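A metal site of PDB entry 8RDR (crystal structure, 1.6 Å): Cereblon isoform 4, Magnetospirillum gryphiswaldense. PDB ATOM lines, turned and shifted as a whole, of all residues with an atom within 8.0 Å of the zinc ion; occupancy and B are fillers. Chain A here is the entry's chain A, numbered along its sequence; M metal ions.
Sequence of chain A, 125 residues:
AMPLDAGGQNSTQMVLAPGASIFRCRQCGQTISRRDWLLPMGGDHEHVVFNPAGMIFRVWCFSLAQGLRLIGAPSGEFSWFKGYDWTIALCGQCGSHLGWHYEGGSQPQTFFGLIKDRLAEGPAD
SG of Cys 94 is bound to the zinc ion (2.3 Å). SG of Cys 28 is bound to the zinc ion, at 2.3 Å. SG of Cys 25 is bound to the zinc ion, 2.4 Å away. The side-chain sulfur (SG) of Cys 91 binds the zinc ion (2.4 Å).
The nearest printed residue that does not touch the zinc ion is Ser 96 (4.4 Å).
The side-chain sulfur (SG) of Cys 28 sits close to the backbone NH (N) of Gln 30 (3.5 Å). The side-chain sulfur (SG) of Cys 94 sits close to the backbone NH (N) of Ser 96 (3.4 Å). The side-chain amide nitrogen (NE2) of Gln 93 sits close to the side-chain sulfur (SG) of Cys 28, 3.3 Å away. The backbone NH (N) of Gln 93 lies close to the side-chain sulfur (SG) of Cys 91. The backbone NH (N) of Gln 27 sits close to the side-chain sulfur (SG) of Cys 25 (3.4 Å). The backbone NH (N) of Cys 91 lies within hydrogen-bond range of the backbone carbonyl oxygen (O) of Ser 96 (2.7 Å). The backbone carbonyl oxygen of Gln 30 sits at hydrogen-bond distance from the backbone NH of Cys 25 (2.8 Å).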
ATOM      1  N   ARG A  24      35.397  25.083  29.511  1.00  0.00           N
ATOM      2  CA  ARG A  24      34.698  24.642  28.305  1.00  0.00           C
ATOM      3  C   ARG A  24      33.245  25.000  28.406  1.00  0.00           C
ATOM      4  O   ARG A  24      32.720  25.117  29.537  1.00  0.00           O
ATOM      5  CB  ARG A  24      34.870  23.128  28.102  1.00  0.00           C
ATOM      6  CG  ARG A  24      36.300  22.726  27.795  1.00  0.00           C
ATOM      7  CD  ARG A  24      36.485  21.238  27.519  1.00  0.00           C
ATOM      8  NE  ARG A  24      37.873  20.998  27.169  1.00  0.00           N
ATOM      9  CZ  ARG A  24      38.442  21.306  26.025  1.00  0.00           C
ATOM     10  NH1 ARG A  24      37.727  21.729  25.011  1.00  0.00           N
ATOM     11  NH2 ARG A  24      39.744  21.148  25.862  1.00  0.00           N
ATOM     12  N   CYS A  25      32.585  25.116  27.259  1.00  0.00           N
ATOM     13  CA  CYS A  25      31.124  25.242  27.190  1.00  0.00           C
ATOM     14  C   CYS A  25      30.508  24.020  27.874  1.00  0.00           C
ATOM     15  O   CYS A  25      30.849  22.912  27.489  1.00  0.00           O
ATOM     16  CB  CYS A  25      30.654  25.325  25.749  1.00  0.00           C
ATOM     17  SG  CYS A  25      28.840  25.416  25.720  1.00  0.00           S
ATOM     18  N   ARG A  26      29.633  24.202  28.849  1.00  0.00           N
ATOM     19  CA  ARG A  26      28.990  23.113  29.609  1.00  0.00           C
ATOM     20  C   ARG A  26      28.092  22.266  28.664  1.00  0.00           C
ATOM     21  O   ARG A  26      27.894  21.079  28.937  1.00  0.00           O
ATOM     22  CB  ARG A  26      28.189  23.730  30.752  1.00  0.00           C
ATOM     23  CG  ARG A  26      27.416  22.753  31.594  1.00  0.00           C
ATOM     24  CD  ARG A  26      26.746  23.499  32.709  1.00  0.00           C
ATOM     25  NE  ARG A  26      25.920  22.602  33.436  1.00  0.00           N
ATOM     26  CZ  ARG A  26      25.165  22.922  34.467  1.00  0.00           C
ATOM     27  NH1 ARG A  26      25.200  24.164  34.940  1.00  0.00           N
ATOM     28  NH2 ARG A  26      24.449  21.977  35.026  1.00  0.00           N
ATOM     29  N   GLN A  27      27.549  22.881  27.617  1.00  0.00           N
ATOM     30  CA  GLN A  27      26.597  22.184  26.719  1.00  0.00           C
ATOM     31  C   GLN A  27      27.324  21.322  25.685  1.00  0.00           C
ATOM     32  O   GLN A  27      26.743  20.279  25.315  1.00  0.00           O
ATOM     33  CB  GLN A  27      25.634  23.196  26.108  1.00  0.00           C
ATOM     34  CG  GLN A  27      24.782  23.856  27.177  1.00  0.00           C
ATOM     35  CD  GLN A  27      24.088  22.868  28.079  1.00  0.00           C
ATOM     36  OE1 GLN A  27      24.071  23.011  29.299  1.00  0.00           O
ATOM     37  NE2 GLN A  27      23.510  21.846  27.493  1.00  0.00           N
ATOM     38  N   CYS A  28      28.531  21.627  25.243  1.00  0.00           N
ATOM     39  CA  CYS A  28      29.127  20.938  24.066  1.00  0.00           C
ATOM     40  C   CYS A  28      30.607  20.658  24.223  1.00  0.00           C
ATOM     41  O   CYS A  28      31.155  19.894  23.381  1.00  0.00           O
ATOM     42  CB  CYS A  28      28.842  21.727  22.805  1.00  0.00           C
ATOM     43  SG  CYS A  28      29.825  23.199  22.656  1.00  0.00           S
ATOM     44  N   GLY A  29      31.322  21.301  25.153  1.00  0.00           N
ATOM     45  CA  GLY A  29      32.762  21.043  25.281  1.00  0.00           C
ATOM     46  C   GLY A  29      33.682  21.981  24.546  1.00  0.00           C
ATOM     47  O   GLY A  29      34.917  21.848  24.705  1.00  0.00           O
ATOM     48  N   GLN A  30      33.149  22.931  23.768  1.00  0.00           N
ATOM     49  CA  GLN A  30      33.979  23.963  23.111  1.00  0.00           C
ATOM     50  C   GLN A  30      34.954  24.580  24.130  1.00  0.00           C
ATOM     51  O   GLN A  30      34.506  24.954  25.211  1.00  0.00           O
ATOM     52  CB  GLN A  30      33.075  25.079  22.567  1.00  0.00           C
ATOM     53  CG  GLN A  30      33.853  26.216  21.945  1.00  0.00           C
ATOM     54  CD  GLN A  30      34.238  25.912  20.523  1.00  0.00           C
ATOM     55  OE1 GLN A  30      34.783  24.850  20.211  1.00  0.00           O
ATOM     56  NE2 GLN A  30      33.950  26.856  19.666  1.00  0.00           N
ATOM     57  N   THR A  31      36.226  24.657  23.797  1.00  0.00           N
ATOM     58  CA  THR A  31      37.225  25.391  24.602  1.00  0.00           C
ATOM     59  C   THR A  31      36.907  26.878  24.622  1.00  0.00           C
ATOM     60  O   THR A  31      36.754  27.454  23.526  1.00  0.00           O
ATOM     61  CB  THR A  31      38.639  25.244  24.013  1.00  0.00           C
ATOM     62  OG1 THR A  31      38.877  23.894  23.574  1.00  0.00           O
ATOM     63  CG2 THR A  31      39.672  25.675  25.026  1.00  0.00           C
ATOM     64  N   ILE A  32      36.781  27.488  25.817  1.00  0.00           N
ATOM     65  CA  ILE A  32      36.367  28.907  25.947  1.00  0.00           C
ATOM     66  C   ILE A  32      37.423  29.759  26.648  1.00  0.00           C
ATOM     67  O   ILE A  32      37.766  30.836  26.132  1.00  0.00           O
ATOM     68  CB  ILE A  32      35.012  29.044  26.644  1.00  0.00           C
ATOM     69  CG1 ILE A  32      33.911  28.248  25.938  1.00  0.00           C
ATOM     70  CG2 ILE A  32      34.663  30.503  26.782  1.00  0.00           C
ATOM     71  CD1 ILE A  32      33.582  28.738  24.521  1.00  0.00           C
ATOM     72  N   GLY A  67      36.659  30.621  21.087  1.00  0.00           N
ATOM     73  CA  GLY A  67      35.580  29.662  20.798  1.00  0.00           C
ATOM     74  C   GLY A  67      34.197  30.283  20.838  1.00  0.00           C
ATOM     75  O   GLY A  67      33.226  29.543  20.849  1.00  0.00           O
ATOM     76  N   LEU A  90      28.010  34.144  22.116  1.00  0.00           N
ATOM     77  CA  LEU A  90      27.509  32.752  22.083  1.00  0.00           C
ATOM     78  C   LEU A  90      28.690  31.798  22.022  1.00  0.00           C
ATOM     79  O   LEU A  90      29.734  32.147  21.465  1.00  0.00           O
ATOM     80  CB  LEU A  90      26.616  32.579  20.868  1.00  0.00           C
ATOM     81  CG  LEU A  90      25.429  33.537  20.771  1.00  0.00           C
ATOM     82  CD1 LEU A  90      24.594  33.192  19.568  1.00  0.00           C
ATOM     83  CD2 LEU A  90      24.618  33.567  22.056  1.00  0.00           C
ATOM     84  N   CYS A  91      28.490  30.579  22.503  1.00  0.00           N
ATOM     85  CA  CYS A  91      29.390  29.460  22.186  1.00  0.00           C
ATOM     86  C   CYS A  91      29.432  29.387  20.659  1.00  0.00           C
ATOM     87  O   CYS A  91      28.328  29.250  20.005  1.00  0.00           O
ATOM     88  CB  CYS A  91      28.884  28.157  22.762  1.00  0.00           C
ATOM     89  SG  CYS A  91      29.951  26.799  22.292  1.00  0.00           S
ATOM     90  N   GLY A  92      30.623  29.447  20.040  1.00  0.00           N
ATOM     91  CA  GLY A  92      30.748  29.422  18.589  1.00  0.00           C
ATOM     92  C   GLY A  92      30.409  28.040  18.004  1.00  0.00           C
ATOM     93  O   GLY A  92      30.191  27.956  16.817  1.00  0.00           O
ATOM     94  N   GLN A  93      30.364  27.014  18.835  1.00  0.00           N
ATOM     95  CA  GLN A  93      30.053  25.647  18.398  1.00  0.00           C
ATOM     96  C   GLN A  93      28.549  25.422  18.513  1.00  0.00           C
ATOM     97  O   GLN A  93      27.932  25.128  17.505  1.00  0.00           O
ATOM     98  CB  GLN A  93      30.913  24.663  19.181  1.00  0.00           C
ATOM     99  CG  GLN A  93      30.695  23.213  18.799  1.00  0.00           C
ATOM    100  CD  GLN A  93      31.877  22.373  19.214  1.00  0.00           C
ATOM    101  OE1 GLN A  93      32.780  22.106  18.444  1.00  0.00           O
ATOM    102  NE2 GLN A  93      31.888  21.902  20.449  1.00  0.00           N
ATOM    103  N   CYS A  94      27.966  25.588  19.696  1.00  0.00           N
ATOM    104  CA  CYS A  94      26.572  25.124  19.944  1.00  0.00           C
ATOM    105  C   CYS A  94      25.574  26.276  20.052  1.00  0.00           C
ATOM    106  O   CYS A  94      24.381  25.982  20.005  1.00  0.00           O
ATOM    107  CB  CYS A  94      26.515  24.235  21.164  1.00  0.00           C
ATOM    108  SG  CYS A  94      26.468  25.121  22.746  1.00  0.00           S
ATOM    109  N   GLY A  95      26.021  27.538  20.109  1.00  0.00           N
ATOM    110  CA  GLY A  95      25.125  28.697  20.195  1.00  0.00           C
ATOM    111  C   GLY A  95      24.610  28.975  21.598  1.00  0.00           C
ATOM    112  O   GLY A  95      23.854  29.961  21.742  1.00  0.00           O
ATOM    113  N   SER A  96      25.037  28.227  22.608  1.00  0.00           N
ATOM    114  CA  SER A  96      24.700  28.518  24.024  1.00  0.00           C
ATOM    115  C   SER A  96      25.099  29.970  24.347  1.00  0.00           C
ATOM    116  O   SER A  96      26.209  30.405  24.007  1.00  0.00           O
ATOM    117  CB  SER A  96      25.411  27.585  24.971  1.00  0.00           C
ATOM    118  OG  SER A  96      25.030  27.857  26.327  1.00  0.00           O
ATOM    119  N   HIS A  97      24.226  30.719  25.018  1.00  0.00           N
ATOM    120  CA  HIS A  97      24.597  32.086  25.432  1.00  0.00           C
ATOM    121  C   HIS A  97      25.560  32.032  26.628  1.00  0.00           C
ATOM    122  O   HIS A  97      25.126  31.687  27.732  1.00  0.00           O
ATOM    123  CB  HIS A  97      23.359  32.905  25.760  1.00  0.00           C
ATOM    124  CG  HIS A  97      23.724  34.266  26.219  1.00  0.00           C
ATOM    125  ND1 HIS A  97      22.891  34.989  27.025  1.00  0.00           N
ATOM    126  CD2 HIS A  97      24.806  35.031  25.947  1.00  0.00           C
ATOM    127  CE1 HIS A  97      23.432  36.191  27.205  1.00  0.00           C
ATOM    128  NE2 HIS A  97      24.648  36.191  26.628  1.00  0.00           N
ATOM    129  N   LEU A  98      26.847  32.312  26.417  1.00  0.00           N
ATOM    130  CA  LEU A  98      27.854  32.142  27.465  1.00  0.00           C
ATOM    131  C   LEU A  98      28.185  33.462  28.162  1.00  0.00           C
ATOM    132  O   LEU A  98      28.736  33.396  29.235  1.00  0.00           O
ATOM    133  CB  LEU A  98      29.104  31.540  26.826  1.00  0.00           C
ATOM    134  CG  LEU A  98      28.956  30.114  26.339  1.00  0.00           C
ATOM    135  CD1 LEU A  98      30.326  29.528  26.008  1.00  0.00           C
ATOM    136  CD2 LEU A  98      28.229  29.200  27.303  1.00  0.00           C
ATOM    137  N   ARG A 118      27.481  28.339  33.090  1.00  0.00           N
ATOM    138  CA  ARG A 118      27.352  27.840  31.708  1.00  0.00           C
ATOM    139  C   ARG A 118      28.678  27.275  31.223  1.00  0.00           C
ATOM    140  O   ARG A 118      28.754  26.915  30.068  1.00  0.00           O
ATOM    141  CB  ARG A 118      26.816  28.949  30.828  1.00  0.00           C
ATOM    142  CG  ARG A 118      25.457  29.381  31.332  1.00  0.00           C
ATOM    143  CD  ARG A 118      24.719  30.271  30.392  1.00  0.00           C
ATOM    144  NE  ARG A 118      23.496  30.673  31.087  1.00  0.00           N
ATOM    145  CZ  ARG A 118      22.544  31.413  30.534  1.00  0.00           C
ATOM    146  NH1 ARG A 118      22.695  31.832  29.290  1.00  0.00           N
ATOM    147  NH2 ARG A 118      21.459  31.737  31.253  1.00  0.00           N
HETATM  148 ZN    ZN M   1      28.686  25.086  23.372  1.00  0.00          ZN
